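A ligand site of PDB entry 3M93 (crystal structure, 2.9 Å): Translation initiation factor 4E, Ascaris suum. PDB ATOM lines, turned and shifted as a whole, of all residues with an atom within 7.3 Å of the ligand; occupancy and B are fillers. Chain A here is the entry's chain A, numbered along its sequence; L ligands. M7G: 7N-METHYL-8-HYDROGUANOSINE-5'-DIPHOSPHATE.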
ATOM      1  N   LEU A  14       9.741   5.517   2.585  1.00  0.00           N
ATOM      2  CA  LEU A  14       9.686   5.194   4.011  1.00  0.00           C
ATOM      3  C   LEU A  14      11.046   4.757   4.501  1.00  0.00           C
ATOM      4  O   LEU A  14      11.557   3.738   4.038  1.00  0.00           O
ATOM      5  CB  LEU A  14       8.642   4.107   4.286  1.00  0.00           C
ATOM      6  CG  LEU A  14       8.409   3.703   5.753  1.00  0.00           C
ATOM      7  CD1 LEU A  14       6.934   3.453   6.010  1.00  0.00           C
ATOM      8  CD2 LEU A  14       9.256   2.503   6.169  1.00  0.00           C
ATOM      9  N   TRP A  22       4.590   3.049  12.194  1.00  0.00           N
ATOM     10  CA  TRP A  22       4.766   2.861  10.758  1.00  0.00           C
ATOM     11  C   TRP A  22       4.268   4.021   9.889  1.00  0.00           C
ATOM     12  O   TRP A  22       5.065   4.663   9.188  1.00  0.00           O
ATOM     13  CB  TRP A  22       4.143   1.533  10.327  1.00  0.00           C
ATOM     14  CG  TRP A  22       4.536   1.118   8.943  1.00  0.00           C
ATOM     15  CD1 TRP A  22       5.687   0.479   8.571  1.00  0.00           C
ATOM     16  CD2 TRP A  22       3.778   1.308   7.739  1.00  0.00           C
ATOM     17  NE1 TRP A  22       5.692   0.256   7.214  1.00  0.00           N
ATOM     18  CE2 TRP A  22       4.534   0.758   6.674  1.00  0.00           C
ATOM     19  CE3 TRP A  22       2.530   1.890   7.453  1.00  0.00           C
ATOM     20  CZ2 TRP A  22       4.086   0.769   5.349  1.00  0.00           C
ATOM     21  CZ3 TRP A  22       2.081   1.901   6.128  1.00  0.00           C
ATOM     22  CH2 TRP A  22       2.855   1.335   5.097  1.00  0.00           C
ATOM     23  N   GLU A  23       2.956   4.286   9.946  1.00  0.00           N
ATOM     24  CA  GLU A  23       2.280   5.293   9.114  1.00  0.00           C
ATOM     25  C   GLU A  23       2.917   6.689   9.041  1.00  0.00           C
ATOM     26  O   GLU A  23       2.787   7.383   8.036  1.00  0.00           O
ATOM     27  CB  GLU A  23       0.831   5.446   9.575  1.00  0.00           C
ATOM     28  CG  GLU A  23      -0.152   4.588   8.810  1.00  0.00           C
ATOM     29  CD  GLU A  23      -1.437   5.337   8.456  1.00  0.00           C
ATOM     30  OE1 GLU A  23      -2.530   4.748   8.608  1.00  0.00           O
ATOM     31  OE2 GLU A  23      -1.347   6.516   8.013  1.00  0.00           O
ATOM     32  N   LEU A  26       5.787   7.145   6.514  1.00  0.00           N
ATOM     33  CA  LEU A  26       5.314   7.057   5.135  1.00  0.00           C
ATOM     34  C   LEU A  26       5.180   8.438   4.509  1.00  0.00           C
ATOM     35  O   LEU A  26       4.187   9.131   4.736  1.00  0.00           O
ATOM     36  CB  LEU A  26       3.960   6.350   5.122  1.00  0.00           C
ATOM     37  CG  LEU A  26       3.534   5.656   3.835  1.00  0.00           C
ATOM     38  CD1 LEU A  26       4.514   4.553   3.491  1.00  0.00           C
ATOM     39  CD2 LEU A  26       2.145   5.081   4.009  1.00  0.00           C
ATOM     40  N   GLY A  54      15.690  -1.435   5.974  1.00  0.00           N
ATOM     41  CA  GLY A  54      14.342  -1.187   6.467  1.00  0.00           C
ATOM     42  C   GLY A  54      13.551  -0.132   5.696  1.00  0.00           C
ATOM     43  O   GLY A  54      12.404   0.160   6.021  1.00  0.00           O
ATOM     44  N   SER A  55      14.172   0.408   4.649  1.00  0.00           N
ATOM     45  CA  SER A  55      13.569   1.458   3.828  1.00  0.00           C
ATOM     46  C   SER A  55      12.832   0.920   2.588  1.00  0.00           C
ATOM     47  O   SER A  55      13.180  -0.150   2.066  1.00  0.00           O
ATOM     48  CB  SER A  55      14.673   2.418   3.409  1.00  0.00           C
ATOM     49  OG  SER A  55      15.553   2.662   4.493  1.00  0.00           O
ATOM     50  N   ASP A  56      11.811   1.666   2.139  1.00  0.00           N
ATOM     51  CA  ASP A  56      11.021   1.354   0.921  1.00  0.00           C
ATOM     52  C   ASP A  56      10.884   2.526  -0.059  1.00  0.00           C
ATOM     53  O   ASP A  56      11.084   3.665   0.309  1.00  0.00           O
ATOM     54  CB  ASP A  56       9.597   0.911   1.283  1.00  0.00           C
ATOM     55  CG  ASP A  56       9.575  -0.076   2.416  1.00  0.00           C
ATOM     56  OD1 ASP A  56       8.857   0.160   3.429  1.00  0.00           O
ATOM     57  OD2 ASP A  56      10.288  -1.100   2.302  1.00  0.00           O
ATOM     58  N   TYR A  58       7.524   3.327  -2.677  1.00  0.00           N
ATOM     59  CA  TYR A  58       6.267   2.929  -3.274  1.00  0.00           C
ATOM     60  C   TYR A  58       5.969   3.857  -4.411  1.00  0.00           C
ATOM     61  O   TYR A  58       6.315   5.031  -4.357  1.00  0.00           O
ATOM     62  CB  TYR A  58       5.134   3.008  -2.260  1.00  0.00           C
ATOM     63  CG  TYR A  58       5.426   2.440  -0.900  1.00  0.00           C
ATOM     64  CD1 TYR A  58       4.921   1.215  -0.519  1.00  0.00           C
ATOM     65  CD2 TYR A  58       6.211   3.148   0.015  1.00  0.00           C
ATOM     66  CE1 TYR A  58       5.182   0.690   0.771  1.00  0.00           C
ATOM     67  CE2 TYR A  58       6.478   2.640   1.293  1.00  0.00           C
ATOM     68  CZ  TYR A  58       5.964   1.416   1.670  1.00  0.00           C
ATOM     69  OH  TYR A  58       6.225   0.896   2.937  1.00  0.00           O
ATOM     70  N   LYS A  65      -3.325   5.318  -0.846  1.00  0.00           N
ATOM     71  CA  LYS A  65      -2.279   5.240   0.178  1.00  0.00           C
ATOM     72  C   LYS A  65      -1.659   3.849   0.059  1.00  0.00           C
ATOM     73  O   LYS A  65      -2.381   2.861   0.004  1.00  0.00           O
ATOM     74  CB  LYS A  65      -2.869   5.508   1.566  1.00  0.00           C
ATOM     75  N   PRO A  66      -0.315   3.749  -0.025  1.00  0.00           N
ATOM     76  CA  PRO A  66       0.287   2.419  -0.268  1.00  0.00           C
ATOM     77  C   PRO A  66       0.329   1.521   0.950  1.00  0.00           C
ATOM     78  O   PRO A  66       1.408   1.113   1.386  1.00  0.00           O
ATOM     79  CB  PRO A  66       1.711   2.760  -0.739  1.00  0.00           C
ATOM     80  CG  PRO A  66       2.018   4.051  -0.080  1.00  0.00           C
ATOM     81  CD  PRO A  66       0.707   4.807   0.079  1.00  0.00           C
ATOM     82  N   MET A  67      -0.855   1.202   1.500  1.00  0.00           N
ATOM     83  CA  MET A  67      -0.970   0.289   2.629  1.00  0.00           C
ATOM     84  C   MET A  67      -2.143  -0.669   2.456  1.00  0.00           C
ATOM     85  O   MET A  67      -2.985  -0.490   1.575  1.00  0.00           O
ATOM     86  CB  MET A  67      -1.071   1.050   3.945  1.00  0.00           C
ATOM     87  CG  MET A  67      -2.089   2.171   3.965  1.00  0.00           C
ATOM     88  SD  MET A  67      -1.863   3.231   5.420  1.00  0.00           S
ATOM     89  CE  MET A  67      -3.364   4.222   5.324  1.00  0.00           C
ATOM     90  N   TRP A  68      -2.167  -1.710   3.298  1.00  0.00           N
ATOM     91  CA  TRP A  68      -3.161  -2.765   3.228  1.00  0.00           C
ATOM     92  C   TRP A  68      -4.552  -2.242   3.511  1.00  0.00           C
ATOM     93  O   TRP A  68      -5.491  -2.545   2.786  1.00  0.00           O
ATOM     94  CB  TRP A  68      -2.873  -3.868   4.248  1.00  0.00           C
ATOM     95  CG  TRP A  68      -1.497  -4.415   4.211  1.00  0.00           C
ATOM     96  CD1 TRP A  68      -0.735  -4.698   3.094  1.00  0.00           C
ATOM     97  CD2 TRP A  68      -0.705  -4.797   5.344  1.00  0.00           C
ATOM     98  NE1 TRP A  68       0.488  -5.220   3.466  1.00  0.00           N
ATOM     99  CE2 TRP A  68       0.536  -5.289   4.840  1.00  0.00           C
ATOM    100  CE3 TRP A  68      -0.909  -4.768   6.728  1.00  0.00           C
ATOM    101  CZ2 TRP A  68       1.554  -5.745   5.688  1.00  0.00           C
ATOM    102  CZ3 TRP A  68       0.115  -5.217   7.565  1.00  0.00           C
ATOM    103  CH2 TRP A  68       1.333  -5.700   7.038  1.00  0.00           C
ATOM    104  N   GLU A  69      -4.665  -1.461   4.592  1.00  0.00           N
ATOM    105  CA  GLU A  69      -5.954  -0.992   5.102  1.00  0.00           C
ATOM    106  C   GLU A  69      -6.713  -0.150   4.095  1.00  0.00           C
ATOM    107  O   GLU A  69      -7.938  -0.071   4.157  1.00  0.00           O
ATOM    108  CB  GLU A  69      -5.796  -0.196   6.412  1.00  0.00           C
ATOM    109  CG  GLU A  69      -5.242  -0.985   7.607  1.00  0.00           C
ATOM    110  CD  GLU A  69      -3.723  -1.106   7.596  1.00  0.00           C
ATOM    111  OE1 GLU A  69      -3.059  -0.272   6.944  1.00  0.00           O
ATOM    112  OE2 GLU A  69      -3.203  -2.042   8.251  1.00  0.00           O
ATOM    113  N   ASP A  70      -5.980   0.459   3.170  1.00  0.00           N
ATOM    114  CA  ASP A  70      -6.563   1.303   2.140  1.00  0.00           C
ATOM    115  C   ASP A  70      -7.621   0.528   1.377  1.00  0.00           C
ATOM    116  O   ASP A  70      -7.474  -0.673   1.157  1.00  0.00           O
ATOM    117  CB  ASP A  70      -5.479   1.785   1.179  1.00  0.00           C
ATOM    118  CG  ASP A  70      -5.952   2.904   0.275  1.00  0.00           C
ATOM    119  OD1 ASP A  70      -5.528   4.056   0.493  1.00  0.00           O
ATOM    120  OD2 ASP A  70      -6.747   2.635  -0.664  1.00  0.00           O
ATOM    121  N   ARG A  78      -0.509  -9.239  -4.044  1.00  0.00           N
ATOM    122  CA  ARG A  78       0.697  -8.747  -4.694  1.00  0.00           C
ATOM    123  C   ARG A  78       1.497  -9.849  -5.389  1.00  0.00           C
ATOM    124  O   ARG A  78       1.371 -11.034  -5.061  1.00  0.00           O
ATOM    125  CB  ARG A  78       1.597  -8.039  -3.693  1.00  0.00           C
ATOM    126  CG  ARG A  78       2.263  -8.990  -2.734  1.00  0.00           C
ATOM    127  CD  ARG A  78       3.115  -8.274  -1.723  1.00  0.00           C
ATOM    128  NE  ARG A  78       4.142  -9.173  -1.210  1.00  0.00           N
ATOM    129  CZ  ARG A  78       4.745  -9.060  -0.038  1.00  0.00           C
ATOM    130  NH1 ARG A  78       5.662  -9.944   0.309  1.00  0.00           N
ATOM    131  NH2 ARG A  78       4.437  -8.088   0.818  1.00  0.00           N
ATOM    132  N   VAL A 119       6.190  -1.713  -5.110  1.00  0.00           N
ATOM    133  CA  VAL A 119       6.915  -1.541  -3.864  1.00  0.00           C
ATOM    134  C   VAL A 119       8.322  -2.141  -3.997  1.00  0.00           C
ATOM    135  O   VAL A 119       8.510  -3.199  -4.627  1.00  0.00           O
ATOM    136  CB  VAL A 119       6.173  -2.261  -2.714  1.00  0.00           C
ATOM    137  CG1 VAL A 119       6.732  -1.846  -1.389  1.00  0.00           C
ATOM    138  CG2 VAL A 119       4.689  -1.950  -2.757  1.00  0.00           C
ATOM    139  N   ASN A 121      11.265  -3.257  -1.229  1.00  0.00           N
ATOM    140  CA  ASN A 121      11.698  -3.356   0.168  1.00  0.00           C
ATOM    141  C   ASN A 121      13.192  -3.638   0.264  1.00  0.00           C
ATOM    142  O   ASN A 121      13.659  -4.682  -0.201  1.00  0.00           O
ATOM    143  CB  ASN A 121      10.907  -4.440   0.925  1.00  0.00           C
ATOM    144  CG  ASN A 121       9.389  -4.239   0.872  1.00  0.00           C
ATOM    145  OD1 ASN A 121       8.649  -5.183   0.596  1.00  0.00           O
ATOM    146  ND2 ASN A 121       8.929  -3.024   1.152  1.00  0.00           N
ATOM    147  N   VAL A 122      13.951  -2.704   0.831  1.00  0.00           N
ATOM    148  CA  VAL A 122      15.375  -2.928   1.017  1.00  0.00           C
ATOM    149  C   VAL A 122      15.534  -3.603   2.366  1.00  0.00           C
ATOM    150  O   VAL A 122      15.096  -3.056   3.383  1.00  0.00           O
ATOM    151  CB  VAL A 122      16.227  -1.632   0.896  1.00  0.00           C
ATOM    152  CG1 VAL A 122      17.688  -1.931   1.206  1.00  0.00           C
ATOM    153  CG2 VAL A 122      16.134  -1.050  -0.514  1.00  0.00           C
ATOM    154  N   ARG A 123      16.102  -4.803   2.356  1.00  0.00           N
ATOM    155  CA  ARG A 123      16.261  -5.615   3.571  1.00  0.00           C
ATOM    156  C   ARG A 123      17.585  -6.411   3.595  1.00  0.00           C
ATOM    157  O   ARG A 123      18.284  -6.546   2.560  1.00  0.00           O
ATOM    158  CB  ARG A 123      15.053  -6.541   3.767  1.00  0.00           C
ATOM    159  CG  ARG A 123      14.250  -6.285   5.040  1.00  0.00           C
ATOM    160  CD  ARG A 123      12.856  -5.718   4.783  1.00  0.00           C
ATOM    161  NE  ARG A 123      12.872  -4.310   4.363  1.00  0.00           N
ATOM    162  CZ  ARG A 123      11.841  -3.473   4.448  1.00  0.00           C
ATOM    163  NH1 ARG A 123      11.982  -2.227   4.022  1.00  0.00           N
ATOM    164  NH2 ARG A 123      10.677  -3.865   4.946  1.00  0.00           N
ATOM    165  N   GLY A 126      16.820 -10.463   2.484  1.00  0.00           N
ATOM    166  CA  GLY A 126      16.570 -10.314   1.056  1.00  0.00           C
ATOM    167  C   GLY A 126      15.834  -9.047   0.695  1.00  0.00           C
ATOM    168  O   GLY A 126      14.956  -8.592   1.436  1.00  0.00           O
ATOM    169  N   LYS A 128      13.112  -7.243  -1.685  1.00  0.00           N
ATOM    170  CA  LYS A 128      11.851  -7.702  -2.280  1.00  0.00           C
ATOM    171  C   LYS A 128      11.358  -6.678  -3.270  1.00  0.00           C
ATOM    172  O   LYS A 128      11.534  -5.493  -3.058  1.00  0.00           O
ATOM    173  CB  LYS A 128      10.791  -7.918  -1.195  1.00  0.00           C
ATOM    174  CG  LYS A 128      11.127  -9.075  -0.264  1.00  0.00           C
ATOM    175  CD  LYS A 128       9.991  -9.412   0.660  1.00  0.00           C
ATOM    176  CE  LYS A 128      10.076  -8.682   1.999  1.00  0.00           C
ATOM    177  NZ  LYS A 128       9.150  -9.269   3.011  1.00  0.00           N
ATOM    178  N   TRP A 132       1.498  -4.598  -6.409  1.00  0.00           N
ATOM    179  CA  TRP A 132       0.230  -4.706  -5.724  1.00  0.00           C
ATOM    180  C   TRP A 132      -0.974  -4.605  -6.690  1.00  0.00           C
ATOM    181  O   TRP A 132      -1.048  -3.714  -7.528  1.00  0.00           O
ATOM    182  CB  TRP A 132       0.130  -3.611  -4.659  1.00  0.00           C
ATOM    183  CG  TRP A 132       0.926  -3.830  -3.419  1.00  0.00           C
ATOM    184  CD1 TRP A 132       2.093  -4.542  -3.284  1.00  0.00           C
ATOM    185  CD2 TRP A 132       0.637  -3.303  -2.129  1.00  0.00           C
ATOM    186  NE1 TRP A 132       2.535  -4.495  -1.987  1.00  0.00           N
ATOM    187  CE2 TRP A 132       1.667  -3.746  -1.257  1.00  0.00           C
ATOM    188  CE3 TRP A 132      -0.392  -2.501  -1.619  1.00  0.00           C
ATOM    189  CZ2 TRP A 132       1.687  -3.414   0.106  1.00  0.00           C
ATOM    190  CZ3 TRP A 132      -0.373  -2.178  -0.254  1.00  0.00           C
ATOM    191  CH2 TRP A 132       0.658  -2.637   0.589  1.00  0.00           C
HETATM  192  PA  M7G L   1       7.397  -4.930   5.824  1.00  0.00           P
HETATM  193  O1A M7G L   1       7.736  -3.611   5.166  1.00  0.00           O
HETATM  194  O2A M7G L   1       6.111  -5.621   5.400  1.00  0.00           O
HETATM  195  O3A M7G L   1       8.617  -5.997   5.634  1.00  0.00           O
HETATM  196  O5' M7G L   1       7.405  -4.655   7.421  1.00  0.00           O
HETATM  197  PB  M7G L   1       9.368  -6.917   6.769  1.00  0.00           P
HETATM  198  O1B M7G L   1       9.708  -6.127   8.016  1.00  0.00           O
HETATM  199  O2B M7G L   1      10.517  -7.599   6.059  1.00  0.00           O
HETATM  200  O3B M7G L   1       8.289  -8.049   7.164  1.00  0.00           O
HETATM  201  C5' M7G L   1       6.389  -5.062   8.338  1.00  0.00           C
HETATM  202  C4' M7G L   1       6.250  -3.914   9.327  1.00  0.00           C
HETATM  203  O4' M7G L   1       5.752  -2.785   8.623  1.00  0.00           O
HETATM  204  C3' M7G L   1       5.264  -4.183  10.458  1.00  0.00           C
HETATM  205  O3' M7G L   1       5.800  -3.592  11.663  1.00  0.00           O
HETATM  206  C2' M7G L   1       3.973  -3.497  10.038  1.00  0.00           C
HETATM  207  O2' M7G L   1       3.292  -2.869  11.139  1.00  0.00           O
HETATM  208  C1' M7G L   1       4.418  -2.454   9.024  1.00  0.00           C
HETATM  209  N9  M7G L   1       3.584  -2.349   7.806  1.00  0.00           N
HETATM  210  C8  M7G L   1       3.996  -2.557   6.548  1.00  0.00           C
HETATM  211  N7  M7G L   1       2.991  -2.352   5.690  1.00  0.00           N
HETATM  212  CM7 M7G L   1       3.077  -2.494   4.215  1.00  0.00           C
HETATM  213  C5  M7G L   1       1.932  -1.995   6.431  1.00  0.00           C
HETATM  214  C6  M7G L   1       0.645  -1.664   6.034  1.00  0.00           C
HETATM  215  O6  M7G L   1       0.306  -1.667   4.828  1.00  0.00           O
HETATM  216  N1  M7G L   1      -0.239  -1.350   7.010  1.00  0.00           N
HETATM  217  C2  M7G L   1       0.117  -1.340   8.323  1.00  0.00           C
HETATM  218  N2  M7G L   1      -0.793  -1.018   9.263  1.00  0.00           N
HETATM  219  N3  M7G L   1       1.379  -1.659   8.706  1.00  0.00           N
HETATM  220  C4  M7G L   1       2.300  -1.993   7.763  1.00  0.00           C
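The indole nitrogen of Trp 22 lies close to an oxygen (O4') of the ligand (3.4 Å).
An oxygen (O2B) of the ligand is in salt-bridge range of the side-chain amino group (NZ) of Lys 128, 3.7 Å away.
The guanidinium group of Arg 123 is in salt-bridge range of an oxygen (O1A) of the ligand (3.0 Å).
O6 of the ligand lies within hydrogen-bond range of N of Trp 68, at 2.9 Å.
The side-chain carboxylate of Glu 69 is in hydrogen-bond range of a nitrogen (N2) of the ligand (2.8 Å).
Merely in contact with the ligand: Met 67.
Hydrophobic or aromatic side chains that line the ligand: Trp 22, Met 67 and Trp 68.
Along chain A the residues within 4 Å of the ligand span positions 22 to 128.
The nearest printed residue that does not touch the ligand is Asn 121 (4.2 Å).
NH1 of Arg 123 is in salt-bridge range of OD2 of Asp 56 (2.7 Å).
NH1 of Arg 123 lies within hydrogen-bond range of O of Ser 55 (3.1 Å).
NH1 of Arg 123 lies close to O of Gly 54, at 3.1 Å.
The backbone carbonyl oxygen (O) of Lys 128 sits at hydrogen-bond distance from the backbone NH (N) of Asn 121.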
